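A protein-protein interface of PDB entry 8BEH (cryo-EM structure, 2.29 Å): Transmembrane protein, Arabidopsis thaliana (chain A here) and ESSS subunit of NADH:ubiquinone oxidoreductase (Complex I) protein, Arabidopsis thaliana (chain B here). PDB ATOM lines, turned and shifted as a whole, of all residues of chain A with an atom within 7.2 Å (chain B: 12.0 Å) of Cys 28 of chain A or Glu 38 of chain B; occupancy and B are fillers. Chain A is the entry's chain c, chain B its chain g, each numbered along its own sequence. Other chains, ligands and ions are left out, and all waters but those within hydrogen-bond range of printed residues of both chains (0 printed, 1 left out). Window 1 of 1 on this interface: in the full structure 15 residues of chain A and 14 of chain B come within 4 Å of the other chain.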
ATOM      1  N   THR A  23       4.787  11.065   5.041  1.00  0.00           N
ATOM      2  CA  THR A  23       5.666  12.067   5.630  1.00  0.00           C
ATOM      3  C   THR A  23       6.515  11.499   6.759  1.00  0.00           C
ATOM      4  O   THR A  23       7.435  12.177   7.225  1.00  0.00           O
ATOM      5  CB  THR A  23       4.834  13.257   6.118  1.00  0.00           C
ATOM      6  OG1 THR A  23       3.793  13.522   5.172  1.00  0.00           O
ATOM      7  CG2 THR A  23       5.689  14.509   6.231  1.00  0.00           C
ATOM      8  N   GLY A  24       6.240  10.272   7.199  1.00  0.00           N
ATOM      9  CA  GLY A  24       7.099   9.571   8.123  1.00  0.00           C
ATOM     10  C   GLY A  24       6.628   9.516   9.561  1.00  0.00           C
ATOM     11  O   GLY A  24       7.228   8.786  10.352  1.00  0.00           O
ATOM     12  N   GLY A  25       5.593  10.260   9.930  1.00  0.00           N
ATOM     13  CA  GLY A  25       5.099  10.235  11.287  1.00  0.00           C
ATOM     14  C   GLY A  25       5.996  10.974  12.265  1.00  0.00           C
ATOM     15  O   GLY A  25       6.911  11.700  11.873  1.00  0.00           O
ATOM     16  N   PRO A  26       5.756  10.788  13.560  1.00  0.00           N
ATOM     17  CA  PRO A  26       6.470  11.579  14.571  1.00  0.00           C
ATOM     18  C   PRO A  26       7.905  11.123  14.795  1.00  0.00           C
ATOM     19  O   PRO A  26       8.191   9.929  14.904  1.00  0.00           O
ATOM     20  CB  PRO A  26       5.625  11.369  15.833  1.00  0.00           C
ATOM     21  CG  PRO A  26       4.997  10.032  15.633  1.00  0.00           C
ATOM     22  CD  PRO A  26       4.758   9.886  14.162  1.00  0.00           C
ATOM     23  N   ASN A  27       8.806  12.106  14.887  1.00  0.00           N
ATOM     24  CA  ASN A  27      10.214  11.882  15.229  1.00  0.00           C
ATOM     25  C   ASN A  27      10.882  10.914  14.253  1.00  0.00           C
ATOM     26  O   ASN A  27      11.529   9.947  14.648  1.00  0.00           O
ATOM     27  CB  ASN A  27      10.354  11.388  16.671  1.00  0.00           C
ATOM     28  CG  ASN A  27       9.862  12.398  17.684  1.00  0.00           C
ATOM     29  OD1 ASN A  27      10.328  13.532  17.722  1.00  0.00           O
ATOM     30  ND2 ASN A  27       8.895  11.998  18.495  1.00  0.00           N
ATOM     31  N   CYS A  28      10.717  11.186  12.962  1.00  0.00           N
ATOM     32  CA  CYS A  28      11.215  10.296  11.921  1.00  0.00           C
ATOM     33  C   CYS A  28      12.720  10.489  11.738  1.00  0.00           C
ATOM     34  O   CYS A  28      13.177  11.584  11.397  1.00  0.00           O
ATOM     35  CB  CYS A  28      10.467  10.547  10.614  1.00  0.00           C
ATOM     36  SG  CYS A  28      10.890   9.417   9.278  1.00  0.00           S
ATOM     37  N   ARG A  29      13.479   9.418  11.958  1.00  0.00           N
ATOM     38  CA  ARG A  29      14.942   9.423  11.884  1.00  0.00           C
ATOM     39  C   ARG A  29      15.417   8.248  11.040  1.00  0.00           C
ATOM     40  O   ARG A  29      15.997   7.295  11.569  1.00  0.00           O
ATOM     41  CB  ARG A  29      15.547   9.316  13.284  1.00  0.00           C
ATOM     42  CG  ARG A  29      15.225  10.449  14.229  1.00  0.00           C
ATOM     43  CD  ARG A  29      16.087  11.658  13.966  1.00  0.00           C
ATOM     44  NE  ARG A  29      17.490  11.266  13.956  1.00  0.00           N
ATOM     45  CZ  ARG A  29      18.505  12.096  13.774  1.00  0.00           C
ATOM     46  NH1 ARG A  29      18.329  13.404  13.758  1.00  0.00           N
ATOM     47  NH2 ARG A  29      19.732  11.603  13.650  1.00  0.00           N
ATOM     48  N   PRO A  30      15.194   8.278   9.726  1.00  0.00           N
ATOM     49  CA  PRO A  30      15.673   7.173   8.884  1.00  0.00           C
ATOM     50  C   PRO A  30      17.189   7.038   8.960  1.00  0.00           C
ATOM     51  O   PRO A  30      17.919   8.029   9.015  1.00  0.00           O
ATOM     52  CB  PRO A  30      15.201   7.561   7.477  1.00  0.00           C
ATOM     53  CG  PRO A  30      14.895   9.006   7.552  1.00  0.00           C
ATOM     54  CD  PRO A  30      14.476   9.295   8.945  1.00  0.00           C
ATOM     55  N   LYS A  31      17.655   5.787   8.964  1.00  0.00           N
ATOM     56  CA  LYS A  31      19.071   5.517   9.188  1.00  0.00           C
ATOM     57  C   LYS A  31      19.932   6.057   8.053  1.00  0.00           C
ATOM     58  O   LYS A  31      21.025   6.584   8.290  1.00  0.00           O
ATOM     59  CB  LYS A  31      19.296   4.016   9.370  1.00  0.00           C
ATOM     60  CG  LYS A  31      20.726   3.571   9.161  1.00  0.00           C
ATOM     61  CD  LYS A  31      20.788   2.160   8.607  1.00  0.00           C
ATOM     62  CE  LYS A  31      21.512   1.223   9.563  1.00  0.00           C
ATOM     63  NZ  LYS A  31      22.011  -0.004   8.882  1.00  0.00           N
ATOM     64  N   HIS A  32      19.453   5.949   6.819  1.00  0.00           N
ATOM     65  CA  HIS A  32      20.201   6.378   5.640  1.00  0.00           C
ATOM     66  C   HIS A  32      19.724   7.723   5.118  1.00  0.00           C
ATOM     67  O   HIS A  32      19.703   7.951   3.907  1.00  0.00           O
ATOM     68  CB  HIS A  32      20.109   5.316   4.555  1.00  0.00           C
ATOM     69  CG  HIS A  32      20.756   4.021   4.930  1.00  0.00           C
ATOM     70  ND1 HIS A  32      22.072   3.940   5.328  1.00  0.00           N
ATOM     71  CD2 HIS A  32      20.267   2.760   4.977  1.00  0.00           C
ATOM     72  CE1 HIS A  32      22.368   2.681   5.597  1.00  0.00           C
ATOM     73  NE2 HIS A  32      21.292   1.946   5.389  1.00  0.00           N
ATOM     74  N   TRP A  33      19.351   8.637   6.015  1.00  0.00           N
ATOM     75  CA  TRP A  33      18.704   9.869   5.580  1.00  0.00           C
ATOM     76  C   TRP A  33      19.643  10.770   4.783  1.00  0.00           C
ATOM     77  O   TRP A  33      19.176  11.535   3.940  1.00  0.00           O
ATOM     78  CB  TRP A  33      18.125  10.620   6.781  1.00  0.00           C
ATOM     79  CG  TRP A  33      19.139  11.262   7.665  1.00  0.00           C
ATOM     80  CD1 TRP A  33      19.689  10.740   8.795  1.00  0.00           C
ATOM     81  CD2 TRP A  33      19.720  12.561   7.500  1.00  0.00           C
ATOM     82  NE1 TRP A  33      20.578  11.627   9.342  1.00  0.00           N
ATOM     83  CE2 TRP A  33      20.616  12.755   8.567  1.00  0.00           C
ATOM     84  CE3 TRP A  33      19.568  13.577   6.553  1.00  0.00           C
ATOM     85  CZ2 TRP A  33      21.362  13.921   8.713  1.00  0.00           C
ATOM     86  CZ3 TRP A  33      20.308  14.734   6.700  1.00  0.00           C
ATOM     87  CH2 TRP A  33      21.192  14.897   7.771  1.00  0.00           C
ATOM     88  N   SER B  30      24.372  17.240  16.449  1.00  0.00           N
ATOM     89  CA  SER B  30      24.483  15.787  16.442  1.00  0.00           C
ATOM     90  C   SER B  30      23.405  15.171  15.560  1.00  0.00           C
ATOM     91  O   SER B  30      23.567  14.064  15.051  1.00  0.00           O
ATOM     92  CB  SER B  30      24.386  15.231  17.863  1.00  0.00           C
ATOM     93  OG  SER B  30      23.098  15.451  18.411  1.00  0.00           O
ATOM     94  N   ARG B  31      22.303  15.903  15.379  1.00  0.00           N
ATOM     95  CA  ARG B  31      21.231  15.447  14.504  1.00  0.00           C
ATOM     96  C   ARG B  31      21.654  15.397  13.045  1.00  0.00           C
ATOM     97  O   ARG B  31      20.950  14.786  12.234  1.00  0.00           O
ATOM     98  CB  ARG B  31      20.005  16.353  14.647  1.00  0.00           C
ATOM     99  CG  ARG B  31      20.190  17.728  14.031  1.00  0.00           C
ATOM    100  CD  ARG B  31      18.948  18.602  14.145  1.00  0.00           C
ATOM    101  NE  ARG B  31      18.124  18.553  12.942  1.00  0.00           N
ATOM    102  CZ  ARG B  31      16.987  19.214  12.778  1.00  0.00           C
ATOM    103  NH1 ARG B  31      16.539  20.058  13.692  1.00  0.00           N
ATOM    104  NH2 ARG B  31      16.287  19.033  11.663  1.00  0.00           N
ATOM    105  N   TRP B  32      22.778  16.024  12.688  1.00  0.00           N
ATOM    106  CA  TRP B  32      23.250  16.025  11.312  1.00  0.00           C
ATOM    107  C   TRP B  32      24.420  15.085  11.066  1.00  0.00           C
ATOM    108  O   TRP B  32      24.661  14.720   9.912  1.00  0.00           O
ATOM    109  CB  TRP B  32      23.656  17.443  10.885  1.00  0.00           C
ATOM    110  CG  TRP B  32      22.639  18.481  11.218  1.00  0.00           C
ATOM    111  CD1 TRP B  32      22.637  19.299  12.302  1.00  0.00           C
ATOM    112  CD2 TRP B  32      21.465  18.808  10.466  1.00  0.00           C
ATOM    113  NE1 TRP B  32      21.540  20.121  12.274  1.00  0.00           N
ATOM    114  CE2 TRP B  32      20.801  19.837  11.158  1.00  0.00           C
ATOM    115  CE3 TRP B  32      20.916  18.333   9.274  1.00  0.00           C
ATOM    116  CZ2 TRP B  32      19.611  20.398  10.699  1.00  0.00           C
ATOM    117  CZ3 TRP B  32      19.734  18.894   8.820  1.00  0.00           C
ATOM    118  CH2 TRP B  32      19.093  19.911   9.533  1.00  0.00           C
ATOM    119  N   THR B  34      25.091  12.125  13.210  1.00  0.00           N
ATOM    120  CA  THR B  34      24.849  10.788  13.727  1.00  0.00           C
ATOM    121  C   THR B  34      23.625  10.189  13.048  1.00  0.00           C
ATOM    122  O   THR B  34      22.537  10.776  13.116  1.00  0.00           O
ATOM    123  CB  THR B  34      24.642  10.807  15.249  1.00  0.00           C
ATOM    124  OG1 THR B  34      23.803  11.912  15.606  1.00  0.00           O
ATOM    125  CG2 THR B  34      25.979  10.938  15.966  1.00  0.00           C
ATOM    126  N   PRO B  35      23.755   9.038  12.391  1.00  0.00           N
ATOM    127  CA  PRO B  35      22.653   8.523  11.572  1.00  0.00           C
ATOM    128  C   PRO B  35      21.449   8.130  12.415  1.00  0.00           C
ATOM    129  O   PRO B  35      21.544   7.888  13.621  1.00  0.00           O
ATOM    130  CB  PRO B  35      23.266   7.304  10.878  1.00  0.00           C
ATOM    131  CG  PRO B  35      24.352   6.855  11.799  1.00  0.00           C
ATOM    132  CD  PRO B  35      24.874   8.084  12.492  1.00  0.00           C
ATOM    133  N   GLY B  36      20.300   8.071  11.749  1.00  0.00           N
ATOM    134  CA  GLY B  36      19.053   7.783  12.423  1.00  0.00           C
ATOM    135  C   GLY B  36      18.954   6.348  12.897  1.00  0.00           C
ATOM    136  O   GLY B  36      19.764   5.482  12.565  1.00  0.00           O
ATOM    137  N   HIS B  37      17.917   6.093  13.696  1.00  0.00           N
ATOM    138  CA  HIS B  37      17.748   4.804  14.354  1.00  0.00           C
ATOM    139  C   HIS B  37      16.727   3.896  13.682  1.00  0.00           C
ATOM    140  O   HIS B  37      16.722   2.693  13.957  1.00  0.00           O
ATOM    141  CB  HIS B  37      17.349   5.009  15.822  1.00  0.00           C
ATOM    142  CG  HIS B  37      16.123   5.850  16.006  1.00  0.00           C
ATOM    143  ND1 HIS B  37      14.886   5.486  15.517  1.00  0.00           N
ATOM    144  CD2 HIS B  37      15.942   7.035  16.638  1.00  0.00           C
ATOM    145  CE1 HIS B  37      13.999   6.412  15.834  1.00  0.00           C
ATOM    146  NE2 HIS B  37      14.614   7.363  16.515  1.00  0.00           N
ATOM    147  N   GLU B  38      15.870   4.429  12.818  1.00  0.00           N
ATOM    148  CA  GLU B  38      14.866   3.615  12.138  1.00  0.00           C
ATOM    149  C   GLU B  38      15.556   2.780  11.065  1.00  0.00           C
ATOM    150  O   GLU B  38      15.771   3.243   9.943  1.00  0.00           O
ATOM    151  CB  GLU B  38      13.777   4.494  11.531  1.00  0.00           C
ATOM    152  CG  GLU B  38      13.460   5.746  12.328  1.00  0.00           C
ATOM    153  CD  GLU B  38      12.369   6.590  11.692  1.00  0.00           C
ATOM    154  OE1 GLU B  38      12.549   7.067  10.554  1.00  0.00           O
ATOM    155  OE2 GLU B  38      11.329   6.799  12.350  1.00  0.00           O
ATOM    156  N   GLU B  39      15.919   1.543  11.414  1.00  0.00           N
ATOM    157  CA  GLU B  39      16.472   0.632  10.417  1.00  0.00           C
ATOM    158  C   GLU B  39      15.446   0.340   9.334  1.00  0.00           C
ATOM    159  O   GLU B  39      15.781   0.292   8.144  1.00  0.00           O
ATOM    160  CB  GLU B  39      16.934  -0.669  11.076  1.00  0.00           C
ATOM    161  CG  GLU B  39      17.660  -0.494  12.400  1.00  0.00           C
ATOM    162  CD  GLU B  39      16.710  -0.425  13.581  1.00  0.00           C
ATOM    163  OE1 GLU B  39      15.499  -0.659  13.381  1.00  0.00           O
ATOM    164  OE2 GLU B  39      17.171  -0.141  14.707  1.00  0.00           O
ATOM    165  N   ARG B  40      14.195   0.150   9.729  1.00  0.00           N
ATOM    166  CA  ARG B  40      13.067   0.021   8.827  1.00  0.00           C
ATOM    167  C   ARG B  40      12.006   1.028   9.241  1.00  0.00           C
ATOM    168  O   ARG B  40      11.925   1.402  10.414  1.00  0.00           O
ATOM    169  CB  ARG B  40      12.481  -1.401   8.848  1.00  0.00           C
ATOM    170  CG  ARG B  40      13.389  -2.490   8.283  1.00  0.00           C
ATOM    171  CD  ARG B  40      12.731  -3.861   8.290  1.00  0.00           C
ATOM    172  NE  ARG B  40      13.640  -4.896   7.813  1.00  0.00           N
ATOM    173  CZ  ARG B  40      13.369  -6.194   7.821  1.00  0.00           C
ATOM    174  NH1 ARG B  40      12.206  -6.655   8.252  1.00  0.00           N
ATOM    175  NH2 ARG B  40      14.285  -7.050   7.378  1.00  0.00           N
ATOM    176  N   PRO B  41      11.194   1.495   8.299  1.00  0.00           N
ATOM    177  CA  PRO B  41      10.196   2.518   8.629  1.00  0.00           C
ATOM    178  C   PRO B  41       9.125   1.991   9.576  1.00  0.00           C
ATOM    179  O   PRO B  41       8.977   0.786   9.788  1.00  0.00           O
ATOM    180  CB  PRO B  41       9.599   2.878   7.266  1.00  0.00           C
ATOM    181  CG  PRO B  41      10.619   2.444   6.264  1.00  0.00           C
ATOM    182  CD  PRO B  41      11.254   1.227   6.854  1.00  0.00           C
ATOM    183  N   LYS B  42       8.365   2.946  10.125  1.00  0.00           N
ATOM    184  CA  LYS B  42       7.242   2.586  11.026  1.00  0.00           C
ATOM    185  C   LYS B  42       6.015   2.276  10.164  1.00  0.00           C
ATOM    186  O   LYS B  42       5.774   3.016   9.187  1.00  0.00           O
ATOM    187  CB  LYS B  42       6.989   3.708  12.042  1.00  0.00           C
ATOM    188  CG  LYS B  42       6.833   5.110  11.471  1.00  0.00           C
ATOM    189  CD  LYS B  42       6.252   6.108  12.449  1.00  0.00           C
ATOM    190  CE  LYS B  42       7.240   6.605  13.482  1.00  0.00           C
ATOM    191  NZ  LYS B  42       8.274   7.479  12.876  1.00  0.00           N
ATOM    192  N   GLY B  43       5.283   1.218  10.503  1.00  0.00           N
ATOM    193  CA  GLY B  43       4.130   0.786   9.743  1.00  0.00           C
ATOM    194  C   GLY B  43       4.499  -0.054   8.533  1.00  0.00           C
ATOM    195  O   GLY B  43       5.662  -0.319   8.234  1.00  0.00           O
ATOM    196  N   TYR B  44       3.465  -0.480   7.821  1.00  0.00           N
ATOM    197  CA  TYR B  44       3.621  -1.197   6.567  1.00  0.00           C
ATOM    198  C   TYR B  44       2.759  -0.510   5.528  1.00  0.00           C
ATOM    199  O   TYR B  44       1.608  -0.167   5.810  1.00  0.00           O
ATOM    200  CB  TYR B  44       3.223  -2.666   6.708  1.00  0.00           C
ATOM    201  CG  TYR B  44       4.250  -3.464   7.460  1.00  0.00           C
ATOM    202  CD1 TYR B  44       5.555  -3.540   7.009  1.00  0.00           C
ATOM    203  CD2 TYR B  44       3.922  -4.116   8.640  1.00  0.00           C
ATOM    204  CE1 TYR B  44       6.502  -4.246   7.700  1.00  0.00           C
ATOM    205  CE2 TYR B  44       4.867  -4.834   9.338  1.00  0.00           C
ATOM    206  CZ  TYR B  44       6.155  -4.896   8.861  1.00  0.00           C
ATOM    207  OH  TYR B  44       7.108  -5.610   9.547  1.00  0.00           O
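N of Pro 30 of chain A lies close to OE1 of Glu 38 of chain B (3.0 Å). The backbone carbonyl oxygen (O) of Arg 31 of chain B sits at hydrogen-bond distance from the guanidinium group (NH1) of Arg 29 of chain A (3.3 Å). The guanidinium group (NH2) of Arg 29 of chain A is in hydrogen-bond range of the backbone carbonyl oxygen (O) of Thr 34 of chain B (3.0 Å). O of Pro 26 of chain A is in hydrogen-bond range of NZ of Lys 42 of chain B (3.2 Å). O of Gly 24 of chain A sits at hydrogen-bond distance from NZ of Lys 42 of chain B. The backbone carbonyl oxygen (O) of Arg 29 of chain A lies within hydrogen-bond range of the backbone NH (N) of His 37 of chain B (3.1 Å). The backbone carbonyl oxygen of Glu 38 of chain B sits at hydrogen-bond distance from the backbone NH of Lys 31 of chain A (3.3 Å). The side-chain sulfur (SG) of Cys 28 of chain A is in hydrogen-bond range of the side-chain carboxylate (OE1) of Glu 38 of chain B (3.1 Å). N of Arg 29 of chain A lies within hydrogen-bond range of OE1 of Glu 38 of chain B (2.9 Å).
The side-chain carboxylate (OE2) of Glu 38 of chain B lies within salt-bridge range of the side-chain amino group (NZ) of Lys 42 of chain B.
Among the printed residues, pairs that only touch across the chains: Asn 27 of chain A with Glu 38 of chain B (3.9 Å), Arg 29 of chain A with Gly 36 of chain B (3.2 Å), Pro 30 of chain A with Gly 36 of chain B (3.6 Å), Lys 31 of chain A with Pro 35 of chain B (3.5 Å), Lys 31 of chain A with Gly 36 of chain B (3.4 Å), Trp 33 of chain A with Arg 31 of chain B (3.6 Å) and Trp 33 of chain A with Trp 32 of chain B (3.6 Å).
Thr 23 of chain A touches none of the printed residues of chain B. No residue of chain B comes within 4 Å of Gly 25 of chain A. Asn 27 of chain A touches just one residue of chain B: Glu 38. Cys 28 of chain A touches just one residue of chain B: Glu 38. Arg 29 of chain A touches five residues of chain B. Of chain B, only Gly 36 and Glu 38 come within 4 Å of Pro 30 of chain A. Lys 31 of chain A touches just these residues of chain B: Pro 35 (3.5 Å), Gly 36 (3.4 Å) and Glu 38 (3.3 Å). Of the printed residues of chain A, Trp 32 of chain B touches Trp 33 (3.6 Å). Printed residues of chain A within 4 Å of Gly 36 of chain B: Arg 29, Pro 30 and Lys 31. Of the printed residues of chain A, His 37 of chain B touches Arg 29. Glu 38 of chain B touches five residues of chain A. Tyr 44 of chain B touches none of the printed residues of chain A. The nearest printed residue of chain A that does not touch Thr 34 of chain B is Trp 33 of chain A (4.3 Å).
Hydrophobic or aromatic side chains of chain B that line the printed part of chain A: Trp 32, Pro 35 and His 37. Among the printed residues, 16 pairs touch across the chains.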
